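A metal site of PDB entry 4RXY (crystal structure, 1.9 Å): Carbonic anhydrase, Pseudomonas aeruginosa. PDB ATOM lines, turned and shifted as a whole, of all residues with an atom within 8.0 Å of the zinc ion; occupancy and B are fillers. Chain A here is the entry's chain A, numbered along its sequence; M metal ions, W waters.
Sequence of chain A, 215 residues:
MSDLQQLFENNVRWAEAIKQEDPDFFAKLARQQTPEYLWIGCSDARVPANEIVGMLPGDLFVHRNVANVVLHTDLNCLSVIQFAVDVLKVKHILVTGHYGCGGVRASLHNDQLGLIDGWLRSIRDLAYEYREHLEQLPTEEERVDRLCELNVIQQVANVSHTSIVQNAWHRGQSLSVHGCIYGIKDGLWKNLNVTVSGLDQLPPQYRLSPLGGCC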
ATOM      1  N   GLY A  41       7.962 -28.495  26.210  1.00  0.00           N
ATOM      2  CA  GLY A  41       7.177 -27.285  26.389  1.00  0.00           C
ATOM      3  C   GLY A  41       7.750 -26.121  25.631  1.00  0.00           C
ATOM      4  O   GLY A  41       8.731 -26.270  24.899  1.00  0.00           O
ATOM      5  N   CYS A  42       7.118 -24.973  25.783  1.00  0.00           N
ATOM      6  CA  CYS A  42       7.570 -23.775  25.107  1.00  0.00           C
ATOM      7  C   CYS A  42       8.649 -23.054  25.917  1.00  0.00           C
ATOM      8  O   CYS A  42       8.686 -23.145  27.148  1.00  0.00           O
ATOM      9  CB  CYS A  42       6.382 -22.840  24.845  1.00  0.00           C
ATOM     10  SG  CYS A  42       6.823 -21.350  23.881  1.00  0.00           S
ATOM     11  N   SER A  43       9.511 -22.352  25.198  1.00  0.00           N
ATOM     12  CA  SER A  43      10.567 -21.536  25.761  1.00  0.00           C
ATOM     13  C   SER A  43      10.054 -20.317  26.540  1.00  0.00           C
ATOM     14  O   SER A  43      10.799 -19.737  27.342  1.00  0.00           O
ATOM     15  CB  SER A  43      11.481 -21.065  24.614  1.00  0.00           C
ATOM     16  OG  SER A  43      12.128 -22.179  23.996  1.00  0.00           O
ATOM     17  N   ASP A  44       8.812 -19.911  26.270  1.00  0.00           N
ATOM     18  CA  ASP A  44       8.168 -18.761  26.912  1.00  0.00           C
ATOM     19  C   ASP A  44       8.554 -18.696  28.391  1.00  0.00           C
ATOM     20  O   ASP A  44       8.384 -19.660  29.137  1.00  0.00           O
ATOM     21  CB  ASP A  44       6.640 -18.833  26.761  1.00  0.00           C
ATOM     22  CG  ASP A  44       5.920 -17.547  27.251  1.00  0.00           C
ATOM     23  OD1 ASP A  44       5.198 -16.893  26.449  1.00  0.00           O
ATOM     24  OD2 ASP A  44       6.070 -17.181  28.436  1.00  0.00           O
ATOM     25  N   ALA A  45       9.112 -17.551  28.786  1.00  0.00           N
ATOM     26  CA  ALA A  45       9.689 -17.386  30.127  1.00  0.00           C
ATOM     27  C   ALA A  45       8.650 -17.598  31.221  1.00  0.00           C
ATOM     28  O   ALA A  45       9.005 -17.858  32.369  1.00  0.00           O
ATOM     29  CB  ALA A  45      10.316 -16.001  30.262  1.00  0.00           C
ATOM     30  N   ARG A  46       7.380 -17.490  30.865  1.00  0.00           N
ATOM     31  CA  ARG A  46       6.312 -17.605  31.848  1.00  0.00           C
ATOM     32  C   ARG A  46       5.853 -19.040  32.084  1.00  0.00           C
ATOM     33  O   ARG A  46       4.900 -19.274  32.845  1.00  0.00           O
ATOM     34  CB  ARG A  46       5.133 -16.741  31.414  1.00  0.00           C
ATOM     35  CG  ARG A  46       5.473 -15.256  31.456  1.00  0.00           C
ATOM     36  CD  ARG A  46       4.504 -14.432  30.637  1.00  0.00           C
ATOM     37  NE  ARG A  46       4.464 -14.847  29.225  1.00  0.00           N
ATOM     38  CZ  ARG A  46       3.756 -14.200  28.301  1.00  0.00           C
ATOM     39  NH1 ARG A  46       3.055 -13.125  28.634  1.00  0.00           N
ATOM     40  NH2 ARG A  46       3.758 -14.627  27.048  1.00  0.00           N
ATOM     41  N   VAL A  47       6.528 -20.000  31.458  1.00  0.00           N
ATOM     42  CA  VAL A  47       6.108 -21.398  31.579  1.00  0.00           C
ATOM     43  C   VAL A  47       7.243 -22.316  32.057  1.00  0.00           C
ATOM     44  O   VAL A  47       7.622 -23.270  31.378  1.00  0.00           O
ATOM     45  CB  VAL A  47       5.533 -21.904  30.231  1.00  0.00           C
ATOM     46  CG1 VAL A  47       4.724 -23.173  30.451  1.00  0.00           C
ATOM     47  CG2 VAL A  47       4.653 -20.812  29.570  1.00  0.00           C
ATOM     48  N   ASN A  65      11.312 -25.340  23.425  1.00  0.00           N
ATOM     49  CA  ASN A  65      11.601 -24.642  22.178  1.00  0.00           C
ATOM     50  C   ASN A  65      10.426 -23.721  21.858  1.00  0.00           C
ATOM     51  O   ASN A  65       9.420 -23.740  22.581  1.00  0.00           O
ATOM     52  CB  ASN A  65      11.923 -25.631  21.014  1.00  0.00           C
ATOM     53  CG  ASN A  65      10.704 -26.460  20.555  1.00  0.00           C
ATOM     54  OD1 ASN A  65       9.682 -25.923  20.145  1.00  0.00           O
ATOM     55  ND2 ASN A  65      10.858 -27.785  20.530  1.00  0.00           N
ATOM     56  N   VAL A  66      10.529 -22.889  20.825  1.00  0.00           N
ATOM     57  CA  VAL A  66       9.419 -21.986  20.544  1.00  0.00           C
ATOM     58  C   VAL A  66       8.181 -22.751  20.056  1.00  0.00           C
ATOM     59  O   VAL A  66       8.194 -23.406  19.013  1.00  0.00           O
ATOM     60  CB  VAL A  66       9.803 -20.900  19.533  1.00  0.00           C
ATOM     61  CG1 VAL A  66       8.619 -19.958  19.301  1.00  0.00           C
ATOM     62  CG2 VAL A  66      11.006 -20.131  20.044  1.00  0.00           C
ATOM     63  N   ALA A  67       7.121 -22.654  20.846  1.00  0.00           N
ATOM     64  CA  ALA A  67       5.801 -23.234  20.593  1.00  0.00           C
ATOM     65  C   ALA A  67       5.791 -24.770  20.664  1.00  0.00           C
ATOM     66  O   ALA A  67       4.913 -25.404  20.097  1.00  0.00           O
ATOM     67  CB  ALA A  67       5.242 -22.764  19.238  1.00  0.00           C
ATOM     68  N   ASN A  68       6.727 -25.331  21.427  1.00  0.00           N
ATOM     69  CA  ASN A  68       6.737 -26.771  21.774  1.00  0.00           C
ATOM     70  C   ASN A  68       6.478 -27.683  20.564  1.00  0.00           C
ATOM     71  O   ASN A  68       5.605 -28.554  20.564  1.00  0.00           O
ATOM     72  CB  ASN A  68       5.738 -27.091  22.922  1.00  0.00           C
ATOM     73  CG  ASN A  68       4.372 -26.420  22.754  1.00  0.00           C
ATOM     74  OD1 ASN A  68       4.169 -25.271  23.175  1.00  0.00           O
ATOM     75  ND2 ASN A  68       3.414 -27.143  22.170  1.00  0.00           N
ATOM     76  N   THR A  96       3.344 -30.036  26.866  1.00  0.00           N
ATOM     77  CA  THR A  96       2.641 -28.903  27.447  1.00  0.00           C
ATOM     78  C   THR A  96       2.813 -27.643  26.603  1.00  0.00           C
ATOM     79  O   THR A  96       3.912 -27.098  26.483  1.00  0.00           O
ATOM     80  CB  THR A  96       3.138 -28.607  28.877  1.00  0.00           C
ATOM     81  OG1 THR A  96       2.961 -29.760  29.695  1.00  0.00           O
ATOM     82  CG2 THR A  96       2.382 -27.407  29.494  1.00  0.00           C
ATOM     83  N   GLY A  97       1.719 -27.171  26.014  1.00  0.00           N
ATOM     84  CA  GLY A  97       1.701 -25.899  25.306  1.00  0.00           C
ATOM     85  C   GLY A  97       1.157 -24.872  26.279  1.00  0.00           C
ATOM     86  O   GLY A  97       0.930 -25.193  27.454  1.00  0.00           O
ATOM     87  N   HIS A  98       0.947 -23.637  25.842  1.00  0.00           N
ATOM     88  CA  HIS A  98       0.284 -22.660  26.716  1.00  0.00           C
ATOM     89  C   HIS A  98      -0.588 -21.713  25.921  1.00  0.00           C
ATOM     90  O   HIS A  98      -0.352 -21.466  24.733  1.00  0.00           O
ATOM     91  CB  HIS A  98       1.301 -21.865  27.548  1.00  0.00           C
ATOM     92  CG  HIS A  98       2.247 -21.061  26.720  1.00  0.00           C
ATOM     93  ND1 HIS A  98       2.120 -19.702  26.534  1.00  0.00           N
ATOM     94  CD2 HIS A  98       3.338 -21.439  26.000  1.00  0.00           C
ATOM     95  CE1 HIS A  98       3.090 -19.267  25.752  1.00  0.00           C
ATOM     96  NE2 HIS A  98       3.840 -20.301  25.410  1.00  0.00           N
ATOM     97  N   TYR A  99      -1.618 -21.175  26.566  1.00  0.00           N
ATOM     98  CA  TYR A  99      -2.428 -20.154  25.945  1.00  0.00           C
ATOM     99  C   TYR A  99      -1.592 -18.899  25.746  1.00  0.00           C
ATOM    100  O   TYR A  99      -0.642 -18.662  26.490  1.00  0.00           O
ATOM    101  CB  TYR A  99      -3.655 -19.858  26.823  1.00  0.00           C
ATOM    102  CG  TYR A  99      -4.616 -21.020  26.829  1.00  0.00           C
ATOM    103  CD1 TYR A  99      -4.890 -21.715  27.994  1.00  0.00           C
ATOM    104  CD2 TYR A  99      -5.232 -21.436  25.651  1.00  0.00           C
ATOM    105  CE1 TYR A  99      -5.785 -22.793  27.995  1.00  0.00           C
ATOM    106  CE2 TYR A  99      -6.116 -22.505  25.641  1.00  0.00           C
ATOM    107  CZ  TYR A  99      -6.394 -23.169  26.810  1.00  0.00           C
ATOM    108  OH  TYR A  99      -7.278 -24.238  26.801  1.00  0.00           O
ATOM    109  N   GLY A 100      -1.964 -18.089  24.753  1.00  0.00           N
ATOM    110  CA  GLY A 100      -1.273 -16.842  24.461  1.00  0.00           C
ATOM    111  C   GLY A 100       0.148 -17.021  23.955  1.00  0.00           C
ATOM    112  O   GLY A 100       0.987 -16.160  24.138  1.00  0.00           O
ATOM    113  N   CYS A 101       0.415 -18.159  23.304  1.00  0.00           N
ATOM    114  CA  CYS A 101       1.761 -18.470  22.822  1.00  0.00           C
ATOM    115  C   CYS A 101       2.100 -17.598  21.609  1.00  0.00           C
ATOM    116  O   CYS A 101       1.394 -17.617  20.606  1.00  0.00           O
ATOM    117  CB  CYS A 101       1.858 -19.965  22.477  1.00  0.00           C
ATOM    118  SG  CYS A 101       3.440 -20.508  21.835  1.00  0.00           S
ATOM    119  N   GLY A 102       3.186 -16.825  21.717  1.00  0.00           N
ATOM    120  CA  GLY A 102       3.611 -15.949  20.637  1.00  0.00           C
ATOM    121  C   GLY A 102       3.983 -16.693  19.365  1.00  0.00           C
ATOM    122  O   GLY A 102       3.804 -16.191  18.252  1.00  0.00           O
ATOM    123  N   GLY A 103       4.530 -17.897  19.521  1.00  0.00           N
ATOM    124  CA  GLY A 103       4.895 -18.716  18.370  1.00  0.00           C
ATOM    125  C   GLY A 103       3.644 -19.094  17.604  1.00  0.00           C
ATOM    126  O   GLY A 103       3.572 -18.973  16.379  1.00  0.00           O
ATOM    127  N   VAL A 104       2.639 -19.576  18.327  1.00  0.00           N
ATOM    128  CA  VAL A 104       1.354 -19.908  17.721  1.00  0.00           C
ATOM    129  C   VAL A 104       0.721 -18.675  17.090  1.00  0.00           C
ATOM    130  O   VAL A 104       0.240 -18.729  15.944  1.00  0.00           O
ATOM    131  CB  VAL A 104       0.384 -20.504  18.739  1.00  0.00           C
ATOM    132  CG1 VAL A 104      -0.963 -20.727  18.085  1.00  0.00           C
ATOM    133  CG2 VAL A 104       0.946 -21.801  19.285  1.00  0.00           C
ATOM    134  N   ARG A 105       0.715 -17.566  17.834  1.00  0.00           N
ATOM    135  CA  ARG A 105       0.137 -16.310  17.335  1.00  0.00           C
ATOM    136  C   ARG A 105       0.796 -15.876  16.037  1.00  0.00           C
ATOM    137  O   ARG A 105       0.114 -15.479  15.092  1.00  0.00           O
ATOM    138  CB  ARG A 105       0.256 -15.205  18.389  1.00  0.00           C
ATOM    139  CG  ARG A 105      -0.358 -13.858  17.977  1.00  0.00           C
ATOM    140  CD  ARG A 105      -0.496 -12.917  19.170  1.00  0.00           C
ATOM    141  NE  ARG A 105      -1.839 -12.946  19.740  1.00  0.00           N
ATOM    142  CZ  ARG A 105      -2.152 -13.474  20.923  1.00  0.00           C
ATOM    143  NH1 ARG A 105      -1.223 -14.048  21.677  1.00  0.00           N
ATOM    144  NH2 ARG A 105      -3.412 -13.449  21.352  1.00  0.00           N
ATOM    145  N   CYS A 148      -3.532 -22.994  19.904  1.00  0.00           N
ATOM    146  CA  CYS A 148      -2.603 -23.484  20.932  1.00  0.00           C
ATOM    147  C   CYS A 148      -2.984 -24.885  21.387  1.00  0.00           C
ATOM    148  O   CYS A 148      -2.123 -25.751  21.565  1.00  0.00           O
ATOM    149  CB  CYS A 148      -2.579 -22.562  22.143  1.00  0.00           C
ATOM    150  SG  CYS A 148      -1.759 -20.984  21.878  1.00  0.00           S
ATOM    151  N   ASN A 151      -2.405 -27.354  18.548  1.00  0.00           N
ATOM    152  CA  ASN A 151      -0.980 -27.627  18.387  1.00  0.00           C
ATOM    153  C   ASN A 151      -0.522 -28.692  19.372  1.00  0.00           C
ATOM    154  O   ASN A 151       0.138 -29.648  18.984  1.00  0.00           O
ATOM    155  CB  ASN A 151      -0.155 -26.348  18.557  1.00  0.00           C
ATOM    156  CG  ASN A 151       1.324 -26.568  18.302  1.00  0.00           C
ATOM    157  OD1 ASN A 151       1.713 -27.204  17.313  1.00  0.00           O
ATOM    158  ND2 ASN A 151       2.169 -26.026  19.186  1.00  0.00           N
ATOM    159  N   ILE A 184      -1.207 -18.994  31.197  1.00  0.00           N
ATOM    160  CA  ILE A 184      -0.341 -17.954  31.743  1.00  0.00           C
ATOM    161  C   ILE A 184      -1.172 -16.927  32.508  1.00  0.00           C
ATOM    162  O   ILE A 184      -0.643 -16.238  33.376  1.00  0.00           O
ATOM    163  CB  ILE A 184       0.480 -17.239  30.646  1.00  0.00           C
ATOM    164  CG1 ILE A 184      -0.442 -16.627  29.571  1.00  0.00           C
ATOM    165  CG2 ILE A 184       1.485 -18.207  30.009  1.00  0.00           C
ATOM    166  CD1 ILE A 184       0.304 -15.797  28.495  1.00  0.00           C
HETATM  167 ZN    ZN M   1       4.903 -20.156  23.635  1.00  0.00          ZN
HETATM  168  O   HOH W   1       5.877 -18.093  23.304  1.00  0.00           O
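The side-chain sulfur of Cys 42 sits close to the backbone NH of Ala 67 (3.3 Å). The side-chain sulfur (SG) of Cys 42 sits close to the backbone carbonyl oxygen (O) of Asn 65. The backbone NH (N) of Gly 103 sits close to the side-chain sulfur (SG) of Cys 101 (3.7 Å). The backbone NH (N) of Val 104 lies close to the side-chain sulfur (SG) of Cys 101 (3.7 Å). O of His 98 lies within hydrogen-bond range of SG of Cys 148 (3.2 Å). NH2 of Arg 46 is in salt-bridge range of OD1 of Asp 44 (2.8 Å). N of Asp 44 sits close to SG of Cys 42.
Residues that only touch the zinc ion: Asp 44 (3.8 Å). Of the 24 residues printed, 4 come within 4 Å of the zinc ion. Along chain A the residues within 4 Å of the zinc ion span positions 42 to 101.
The zinc ion is bound by NE2 of His 98 (2.1 Å), SG of Cys 42 (2.3 Å), water W1 (2.3 Å) and SG of Cys 101 (2.3 Å).
Water W1 lies within hydrogen-bond range of N of Gly 102 (3.4 Å) and OD1 of Asp 44 (3.4 Å).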
